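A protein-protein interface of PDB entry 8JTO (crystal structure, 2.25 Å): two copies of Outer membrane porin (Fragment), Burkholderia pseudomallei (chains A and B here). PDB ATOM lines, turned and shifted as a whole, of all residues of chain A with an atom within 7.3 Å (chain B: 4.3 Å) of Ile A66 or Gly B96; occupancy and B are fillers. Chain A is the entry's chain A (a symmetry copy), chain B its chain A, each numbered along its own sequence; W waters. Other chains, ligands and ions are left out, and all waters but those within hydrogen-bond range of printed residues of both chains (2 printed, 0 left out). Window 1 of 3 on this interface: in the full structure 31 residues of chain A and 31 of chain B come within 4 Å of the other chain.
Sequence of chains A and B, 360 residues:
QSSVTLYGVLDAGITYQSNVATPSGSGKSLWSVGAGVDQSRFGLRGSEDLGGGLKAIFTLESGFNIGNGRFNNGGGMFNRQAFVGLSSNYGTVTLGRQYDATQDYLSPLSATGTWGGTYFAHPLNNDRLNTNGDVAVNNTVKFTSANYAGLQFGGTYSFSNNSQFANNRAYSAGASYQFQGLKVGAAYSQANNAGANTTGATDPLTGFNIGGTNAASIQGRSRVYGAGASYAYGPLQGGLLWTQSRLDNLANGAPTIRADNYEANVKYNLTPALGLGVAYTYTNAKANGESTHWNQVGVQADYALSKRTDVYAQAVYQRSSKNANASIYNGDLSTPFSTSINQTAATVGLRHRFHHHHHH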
ATOM      1  N   VAL A   9     -36.654 -21.640  -3.981  1.00  0.00           N
ATOM      2  CA  VAL A   9     -35.865 -22.423  -3.036  1.00  0.00           C
ATOM      3  C   VAL A   9     -34.951 -21.456  -2.304  1.00  0.00           C
ATOM      4  O   VAL A   9     -34.236 -20.677  -2.939  1.00  0.00           O
ATOM      5  CB  VAL A   9     -35.034 -23.525  -3.726  1.00  0.00           C
ATOM      6  CG1 VAL A   9     -34.282 -24.353  -2.688  1.00  0.00           C
ATOM      7  CG2 VAL A   9     -35.920 -24.424  -4.577  1.00  0.00           C
ATOM      8  N   LEU A  10     -34.988 -21.491  -0.977  1.00  0.00           N
ATOM      9  CA  LEU A  10     -34.080 -20.723  -0.139  1.00  0.00           C
ATOM     10  C   LEU A  10     -33.160 -21.695   0.582  1.00  0.00           C
ATOM     11  O   LEU A  10     -33.628 -22.620   1.252  1.00  0.00           O
ATOM     12  CB  LEU A  10     -34.836 -19.866   0.877  1.00  0.00           C
ATOM     13  CG  LEU A  10     -35.910 -18.920   0.345  1.00  0.00           C
ATOM     14  CD1 LEU A  10     -37.281 -19.509   0.594  1.00  0.00           C
ATOM     15  CD2 LEU A  10     -35.785 -17.576   1.027  1.00  0.00           C
ATOM     16  N   ASP A  11     -31.860 -21.495   0.419  1.00  0.00           N
ATOM     17  CA  ASP A  11     -30.864 -22.381   0.997  1.00  0.00           C
ATOM     18  C   ASP A  11     -29.811 -21.485   1.621  1.00  0.00           C
ATOM     19  O   ASP A  11     -29.177 -20.689   0.922  1.00  0.00           O
ATOM     20  CB  ASP A  11     -30.259 -23.302  -0.077  1.00  0.00           C
ATOM     21  CG  ASP A  11     -29.180 -24.251   0.469  1.00  0.00           C
ATOM     22  OD1 ASP A  11     -28.508 -23.944   1.484  1.00  0.00           O
ATOM     23  OD2 ASP A  11     -29.004 -25.328  -0.145  1.00  0.00           O
ATOM     24  N   ALA A  12     -29.646 -21.592   2.930  1.00  0.00           N
ATOM     25  CA  ALA A  12     -28.644 -20.809   3.631  1.00  0.00           C
ATOM     26  C   ALA A  12     -27.956 -21.714   4.634  1.00  0.00           C
ATOM     27  O   ALA A  12     -28.603 -22.512   5.316  1.00  0.00           O
ATOM     28  CB  ALA A  12     -29.260 -19.595   4.346  1.00  0.00           C
ATOM     29  N   GLY A  13     -26.640 -21.588   4.715  1.00  0.00           N
ATOM     30  CA  GLY A  13     -25.893 -22.375   5.668  1.00  0.00           C
ATOM     31  C   GLY A  13     -24.611 -21.672   6.040  1.00  0.00           C
ATOM     32  O   GLY A  13     -24.183 -20.711   5.397  1.00  0.00           O
ATOM     33  N   VAL A  33     -21.523 -17.379   5.118  1.00  0.00           N
ATOM     34  CA  VAL A  33     -22.946 -17.684   5.057  1.00  0.00           C
ATOM     35  C   VAL A  33     -23.343 -17.621   3.590  1.00  0.00           C
ATOM     36  O   VAL A  33     -23.010 -16.652   2.895  1.00  0.00           O
ATOM     37  CB  VAL A  33     -23.780 -16.707   5.901  1.00  0.00           C
ATOM     38  CG1 VAL A  33     -25.245 -16.754   5.463  1.00  0.00           C
ATOM     39  CG2 VAL A  33     -23.640 -17.022   7.397  1.00  0.00           C
ATOM     40  N   GLY A  34     -24.030 -18.653   3.118  1.00  0.00           N
ATOM     41  CA  GLY A  34     -24.351 -18.743   1.705  1.00  0.00           C
ATOM     42  C   GLY A  34     -25.083 -20.034   1.428  1.00  0.00           C
ATOM     43  O   GLY A  34     -25.375 -20.818   2.335  1.00  0.00           O
ATOM     44  N   ALA A  35     -25.381 -20.245   0.148  1.00  0.00           N
ATOM     45  CA  ALA A  35     -26.040 -21.476  -0.272  1.00  0.00           C
ATOM     46  C   ALA A  35     -25.160 -22.677   0.050  1.00  0.00           C
ATOM     47  O   ALA A  35     -23.974 -22.705  -0.294  1.00  0.00           O
ATOM     48  CB  ALA A  35     -26.344 -21.432  -1.773  1.00  0.00           C
ATOM     49  N   GLY A  36     -25.736 -23.660   0.731  1.00  0.00           N
ATOM     50  CA  GLY A  36     -25.029 -24.903   0.959  1.00  0.00           C
ATOM     51  C   GLY A  36     -25.208 -25.891  -0.181  1.00  0.00           C
ATOM     52  O   GLY A  36     -24.253 -26.199  -0.895  1.00  0.00           O
ATOM     53  N   GLN A  39     -28.531 -23.542  -5.089  1.00  0.00           N
ATOM     54  CA  GLN A  39     -28.558 -22.094  -5.233  1.00  0.00           C
ATOM     55  C   GLN A  39     -29.969 -21.589  -4.963  1.00  0.00           C
ATOM     56  O   GLN A  39     -30.947 -22.154  -5.467  1.00  0.00           O
ATOM     57  CB  GLN A  39     -28.112 -21.700  -6.642  1.00  0.00           C
ATOM     58  CG  GLN A  39     -28.012 -20.208  -6.898  1.00  0.00           C
ATOM     59  CD  GLN A  39     -27.639 -19.909  -8.343  1.00  0.00           C
ATOM     60  OE1 GLN A  39     -28.482 -19.981  -9.235  1.00  0.00           O
ATOM     61  NE2 GLN A  39     -26.371 -19.595  -8.579  1.00  0.00           N
ATOM     62  N   SER A  40     -30.092 -20.547  -4.144  1.00  0.00           N
ATOM     63  CA  SER A  40     -31.413 -19.972  -3.939  1.00  0.00           C
ATOM     64  C   SER A  40     -31.935 -19.406  -5.254  1.00  0.00           C
ATOM     65  O   SER A  40     -31.171 -18.920  -6.095  1.00  0.00           O
ATOM     66  CB  SER A  40     -31.381 -18.887  -2.857  1.00  0.00           C
ATOM     67  OG  SER A  40     -31.094 -19.462  -1.586  1.00  0.00           O
ATOM     68  N   PHE A  64     -30.160 -16.284  -7.006  1.00  0.00           N
ATOM     69  CA  PHE A  64     -29.636 -15.182  -6.211  1.00  0.00           C
ATOM     70  C   PHE A  64     -28.920 -15.737  -4.991  1.00  0.00           C
ATOM     71  O   PHE A  64     -29.135 -16.882  -4.583  1.00  0.00           O
ATOM     72  CB  PHE A  64     -30.752 -14.210  -5.782  1.00  0.00           C
ATOM     73  CG  PHE A  64     -31.766 -14.813  -4.833  1.00  0.00           C
ATOM     74  CD1 PHE A  64     -32.840 -15.545  -5.315  1.00  0.00           C
ATOM     75  CD2 PHE A  64     -31.647 -14.632  -3.464  1.00  0.00           C
ATOM     76  CE1 PHE A  64     -33.780 -16.093  -4.449  1.00  0.00           C
ATOM     77  CE2 PHE A  64     -32.571 -15.174  -2.591  1.00  0.00           C
ATOM     78  CZ  PHE A  64     -33.640 -15.912  -3.084  1.00  0.00           C
ATOM     79  N   ASN A  65     -28.075 -14.884  -4.413  1.00  0.00           N
ATOM     80  CA  ASN A  65     -27.322 -15.172  -3.198  1.00  0.00           C
ATOM     81  C   ASN A  65     -28.125 -14.702  -1.989  1.00  0.00           C
ATOM     82  O   ASN A  65     -28.350 -13.499  -1.812  1.00  0.00           O
ATOM     83  CB  ASN A  65     -25.962 -14.477  -3.247  1.00  0.00           C
ATOM     84  CG  ASN A  65     -25.003 -14.977  -2.176  1.00  0.00           C
ATOM     85  OD1 ASN A  65     -25.420 -15.393  -1.090  1.00  0.00           O
ATOM     86  ND2 ASN A  65     -23.710 -14.941  -2.476  1.00  0.00           N
ATOM     87  N   ILE A  66     -28.545 -15.648  -1.150  1.00  0.00           N
ATOM     88  CA  ILE A  66     -29.282 -15.305   0.067  1.00  0.00           C
ATOM     89  C   ILE A  66     -28.415 -14.476   1.010  1.00  0.00           C
ATOM     90  O   ILE A  66     -28.934 -13.702   1.827  1.00  0.00           O
ATOM     91  CB  ILE A  66     -29.786 -16.588   0.761  1.00  0.00           C
ATOM     92  CG1 ILE A  66     -30.811 -16.268   1.857  1.00  0.00           C
ATOM     93  CG2 ILE A  66     -28.595 -17.377   1.335  1.00  0.00           C
ATOM     94  CD1 ILE A  66     -32.237 -16.071   1.373  1.00  0.00           C
ATOM     95  N   GLY A  67     -27.090 -14.613   0.908  1.00  0.00           N
ATOM     96  CA  GLY A  67     -26.203 -13.888   1.804  1.00  0.00           C
ATOM     97  C   GLY A  67     -26.225 -12.382   1.591  1.00  0.00           C
ATOM     98  O   GLY A  67     -26.159 -11.615   2.547  1.00  0.00           O
ATOM     99  N   ASN A  68     -26.310 -11.939   0.333  1.00  0.00           N
ATOM    100  CA  ASN A  68     -26.281 -10.515   0.025  1.00  0.00           C
ATOM    101  C   ASN A  68     -27.440 -10.039  -0.849  1.00  0.00           C
ATOM    102  O   ASN A  68     -27.452  -8.865  -1.236  1.00  0.00           O
ATOM    103  CB  ASN A  68     -24.951 -10.143  -0.655  1.00  0.00           C
ATOM    104  CG  ASN A  68     -24.667 -10.996  -1.892  1.00  0.00           C
ATOM    105  OD1 ASN A  68     -25.589 -11.406  -2.608  1.00  0.00           O
ATOM    106  ND2 ASN A  68     -23.389 -11.271  -2.142  1.00  0.00           N
ATOM    107  N   GLY A  69     -28.395 -10.910  -1.191  1.00  0.00           N
ATOM    108  CA  GLY A  69     -29.543 -10.527  -1.993  1.00  0.00           C
ATOM    109  C   GLY A  69     -29.277 -10.263  -3.469  1.00  0.00           C
ATOM    110  O   GLY A  69     -30.215  -9.889  -4.187  1.00  0.00           O
ATOM    111  N   ARG A  70     -28.049 -10.455  -3.956  1.00  0.00           N
ATOM    112  CA  ARG A  70     -27.710 -10.120  -5.336  1.00  0.00           C
ATOM    113  C   ARG A  70     -27.981 -11.291  -6.280  1.00  0.00           C
ATOM    114  O   ARG A  70     -27.876 -12.457  -5.895  1.00  0.00           O
ATOM    115  CB  ARG A  70     -26.236  -9.708  -5.447  1.00  0.00           C
ATOM    116  CG  ARG A  70     -25.781  -8.701  -4.393  1.00  0.00           C
ATOM    117  CD  ARG A  70     -24.331  -8.243  -4.608  1.00  0.00           C
ATOM    118  NE  ARG A  70     -23.838  -7.509  -3.444  1.00  0.00           N
ATOM    119  CZ  ARG A  70     -22.642  -7.674  -2.892  1.00  0.00           C
ATOM    120  NH1 ARG A  70     -21.753  -8.518  -3.397  1.00  0.00           N
ATOM    121  NH2 ARG A  70     -22.322  -6.962  -1.814  1.00  0.00           N
ATOM    122  N   ASN A  72     -26.899 -13.868  -9.071  1.00  0.00           N
ATOM    123  CA  ASN A  72     -25.631 -14.446  -9.495  1.00  0.00           C
ATOM    124  C   ASN A  72     -25.802 -15.002 -10.903  1.00  0.00           C
ATOM    125  O   ASN A  72     -26.671 -14.527 -11.642  1.00  0.00           O
ATOM    126  CB  ASN A  72     -25.147 -15.505  -8.504  1.00  0.00           C
ATOM    127  CG  ASN A  72     -26.256 -16.353  -7.988  1.00  0.00           C
ATOM    128  OD1 ASN A  72     -27.241 -16.592  -8.688  1.00  0.00           O
ATOM    129  ND2 ASN A  72     -26.116 -16.828  -6.758  1.00  0.00           N
ATOM    130  N   LEU B  60     -38.175 -12.230   1.442  1.00  0.00           N
ATOM    131  CA  LEU B  60     -37.405 -11.744   0.306  1.00  0.00           C
ATOM    132  C   LEU B  60     -38.007 -10.393  -0.050  1.00  0.00           C
ATOM    133  O   LEU B  60     -39.158 -10.327  -0.485  1.00  0.00           O
ATOM    134  CB  LEU B  60     -37.465 -12.722  -0.869  1.00  0.00           C
ATOM    135  CG  LEU B  60     -36.982 -14.155  -0.614  1.00  0.00           C
ATOM    136  CD1 LEU B  60     -37.426 -15.087  -1.740  1.00  0.00           C
ATOM    137  CD2 LEU B  60     -35.468 -14.191  -0.441  1.00  0.00           C
ATOM    138  N   ALA B  82     -33.166 -10.509   2.720  1.00  0.00           N
ATOM    139  CA  ALA B  82     -33.274 -11.824   2.095  1.00  0.00           C
ATOM    140  C   ALA B  82     -32.793 -12.840   3.122  1.00  0.00           C
ATOM    141  O   ALA B  82     -31.591 -12.939   3.379  1.00  0.00           O
ATOM    142  CB  ALA B  82     -32.458 -11.897   0.806  1.00  0.00           C
ATOM    143  N   PHE B  83     -33.717 -13.570   3.738  1.00  0.00           N
ATOM    144  CA  PHE B  83     -33.299 -14.494   4.776  1.00  0.00           C
ATOM    145  C   PHE B  83     -34.273 -15.657   4.887  1.00  0.00           C
ATOM    146  O   PHE B  83     -35.415 -15.604   4.416  1.00  0.00           O
ATOM    147  CB  PHE B  83     -33.125 -13.781   6.127  1.00  0.00           C
ATOM    148  CG  PHE B  83     -34.387 -13.188   6.680  1.00  0.00           C
ATOM    149  CD1 PHE B  83     -35.285 -13.970   7.392  1.00  0.00           C
ATOM    150  CD2 PHE B  83     -34.658 -11.833   6.522  1.00  0.00           C
ATOM    151  CE1 PHE B  83     -36.451 -13.423   7.913  1.00  0.00           C
ATOM    152  CE2 PHE B  83     -35.818 -11.272   7.052  1.00  0.00           C
ATOM    153  CZ  PHE B  83     -36.715 -12.065   7.744  1.00  0.00           C
ATOM    154  N   LEU B  95     -30.964 -16.550   8.713  1.00  0.00           N
ATOM    155  CA  LEU B  95     -29.724 -16.456   7.948  1.00  0.00           C
ATOM    156  C   LEU B  95     -29.963 -15.715   6.642  1.00  0.00           C
ATOM    157  O   LEU B  95     -30.879 -16.063   5.891  1.00  0.00           O
ATOM    158  CB  LEU B  95     -29.175 -17.847   7.629  1.00  0.00           C
ATOM    159  CG  LEU B  95     -28.428 -18.570   8.745  1.00  0.00           C
ATOM    160  CD1 LEU B  95     -28.774 -20.038   8.723  1.00  0.00           C
ATOM    161  CD2 LEU B  95     -26.957 -18.377   8.518  1.00  0.00           C
ATOM    162  N   GLY B  96     -29.116 -14.732   6.353  1.00  0.00           N
ATOM    163  CA  GLY B  96     -29.112 -14.035   5.086  1.00  0.00           C
ATOM    164  C   GLY B  96     -28.834 -12.556   5.287  1.00  0.00           C
ATOM    165  O   GLY B  96     -28.249 -12.153   6.289  1.00  0.00           O
ATOM    166  N   ARG B  97     -29.252 -11.750   4.310  1.00  0.00           N
ATOM    167  CA  ARG B  97     -29.107 -10.298   4.381  1.00  0.00           C
ATOM    168  C   ARG B  97     -30.231  -9.712   5.229  1.00  0.00           C
ATOM    169  O   ARG B  97     -31.413  -9.866   4.905  1.00  0.00           O
ATOM    170  CB  ARG B  97     -29.117  -9.697   2.978  1.00  0.00           C
ATOM    171  CG  ARG B  97     -29.077  -8.156   2.935  1.00  0.00           C
ATOM    172  CD  ARG B  97     -29.041  -7.701   1.480  1.00  0.00           C
ATOM    173  NE  ARG B  97     -29.194  -6.259   1.328  1.00  0.00           N
ATOM    174  CZ  ARG B  97     -28.192  -5.404   1.167  1.00  0.00           C
ATOM    175  NH1 ARG B  97     -26.928  -5.801   1.194  1.00  0.00           N
ATOM    176  NH2 ARG B  97     -28.465  -4.117   0.970  1.00  0.00           N
ATOM    177  N   GLN B  98     -29.863  -9.042   6.315  1.00  0.00           N
ATOM    178  CA  GLN B  98     -30.809  -8.696   7.359  1.00  0.00           C
ATOM    179  C   GLN B  98     -30.464  -7.331   7.941  1.00  0.00           C
ATOM    180  O   GLN B  98     -29.306  -6.916   7.933  1.00  0.00           O
ATOM    181  CB  GLN B  98     -30.803  -9.755   8.476  1.00  0.00           C
ATOM    182  CG  GLN B  98     -31.222 -11.145   8.017  1.00  0.00           C
ATOM    183  CD  GLN B  98     -31.231 -12.168   9.151  1.00  0.00           C
ATOM    184  OE1 GLN B  98     -32.171 -12.211   9.938  1.00  0.00           O
ATOM    185  NE2 GLN B  98     -30.182 -12.995   9.233  1.00  0.00           N
ATOM    186  N   VAL B 137     -27.239  -5.715   6.536  1.00  0.00           N
ATOM    187  CA  VAL B 137     -25.923  -6.355   6.615  1.00  0.00           C
ATOM    188  C   VAL B 137     -25.999  -7.741   5.989  1.00  0.00           C
ATOM    189  O   VAL B 137     -26.935  -8.506   6.251  1.00  0.00           O
ATOM    190  CB  VAL B 137     -25.372  -6.465   8.059  1.00  0.00           C
ATOM    191  CG1 VAL B 137     -24.594  -5.213   8.444  1.00  0.00           C
ATOM    192  CG2 VAL B 137     -26.470  -6.757   9.054  1.00  0.00           C
ATOM    193  N   ASN B 139     -24.682 -11.673   4.975  1.00  0.00           N
ATOM    194  CA  ASN B 139     -24.037 -12.857   5.545  1.00  0.00           C
ATOM    195  C   ASN B 139     -24.329 -12.980   7.035  1.00  0.00           C
ATOM    196  O   ASN B 139     -23.470 -13.385   7.821  1.00  0.00           O
ATOM    197  CB  ASN B 139     -22.523 -12.833   5.291  1.00  0.00           C
ATOM    198  CG  ASN B 139     -22.175 -12.425   3.863  1.00  0.00           C
ATOM    199  OD1 ASN B 139     -22.862 -12.804   2.918  1.00  0.00           O
ATOM    200  ND2 ASN B 139     -21.115 -11.638   3.706  1.00  0.00           N
ATOM    201  N   THR B 140     -25.547 -12.629   7.429  1.00  0.00           N
ATOM    202  CA  THR B 140     -25.875 -12.432   8.835  1.00  0.00           C
ATOM    203  C   THR B 140     -26.553 -13.664   9.425  1.00  0.00           C
ATOM    204  O   THR B 140     -27.486 -14.218   8.829  1.00  0.00           O
ATOM    205  CB  THR B 140     -26.770 -11.198   8.999  1.00  0.00           C
ATOM    206  OG1 THR B 140     -26.067 -10.049   8.518  1.00  0.00           O
ATOM    207  CG2 THR B 140     -27.139 -10.980  10.459  1.00  0.00           C
HETATM  208  O   HOH W   1     -25.646  -6.540  -1.521  1.00  0.00           O
HETATM  209  O   HOH W   2     -21.955 -12.395   0.266  1.00  0.00           O
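Among the printed residues, pairs that only touch across the chains: Leu A10 with Leu B60 (3.7 Å), Leu A10 with Phe B83 (3.9 Å), Ala A12 with Leu B95 (3.7 Å), Val A33 with Leu B95 (3.8 Å), Val A33 with Asn B139 (3.7 Å), Phe A64 with Leu B60 (3.6 Å), Ile A66 with Phe B83 (3.7 Å), Ile A66 with Gly B96 (3.3 Å), Gly A67 with Gly B96 (3.9 Å), Gly A67 with Arg B97 (3.6 Å) and Asn A68 with Arg B97 (3.4 Å).
Water W1 lies within hydrogen-bond range of NE of Arg A70, O of Asn A68 and NH1 of Arg B97. Water W2 lies within hydrogen-bond range of the side-chain amide oxygen (OD1) of Asn B139 (2.8 Å) and the side-chain amide nitrogen (ND2) of Asn A68 (3.0 Å).
Of the printed residues of chain A, Gly B96 touches Ile A66 and Gly A67. Of the printed residues of chain A, Phe B83 touches Leu A10 and Ile A66. Printed residues of chain A within 4 Å of Ala B82: Ile A66 (3.2 Å). Of the printed residues of chain B, Ala A12 touches Leu B95. Printed residues of chain B within 4 Å of Phe A64: Leu B60 (3.6 Å). Printed residues of chain B within 4 Å of Leu A10: Leu B60 (3.7 Å) and Phe B83 (3.9 Å). Gly A36 touches none of the printed residues of chain B. The nearest residue of chain A that does not touch Gly B96 is Val A33 (4.5 Å).
The backbone NH (N) of Arg A70 sits at hydrogen-bond distance from the side-chain amide oxygen (OD1) of Asn A68, at 3.0 Å. O of Gly B96 lies within hydrogen-bond range of N of Thr B140 (3.0 Å). The backbone carbonyl oxygen (O) of Ser A40 sits at hydrogen-bond distance from the backbone NH (N) of Phe A64, 3.0 Å away. The side-chain amide oxygen of Asn A72 lies within hydrogen-bond range of the backbone NH of Phe A64 (3.4 Å). The backbone NH (N) of Arg B97 sits at hydrogen-bond distance from the backbone carbonyl oxygen (O) of Ala B82 (2.8 Å). The side-chain amide oxygen (OD1) of Asn A65 sits at hydrogen-bond distance from the backbone NH (N) of Gly A67 (2.7 Å).
The backbone NH of Arg B97 is in hydrogen-bond range of the backbone carbonyl oxygen of Ile A66 (3.2 Å). O of Ile A66 sits close to O of Ala B82, at 3.2 Å. The backbone carbonyl oxygen (O) of Gly A67 lies within hydrogen-bond range of the backbone NH (N) of Asn B139.
No position is printed for both chains.
Of the 19 printed residues of chain A, 7 touch a printed residue of chain B. Hydrophobic or aromatic side chains of chain A within 4 Å of the printed part of chain B: Leu A10, Ala A12, Val A33, Phe A64 and Ile A66. Printed residues of chain B that touch a printed residue of chain A: Leu B60, Ala B82, Phe B83, Leu B95, Gly B96, Arg B97 and Asn B139. Hydrophobic or aromatic side chains of chain B within 4 Å of the printed part of chain A: Leu B60 and Leu B95. Along chain B the printed residues that touch a printed residue of chain A span positions 60 to 139. Among the printed residues, no Asp or Glu carboxylate lies within 4 Å of a Lys or Arg side-chain nitrogen of the other chain.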
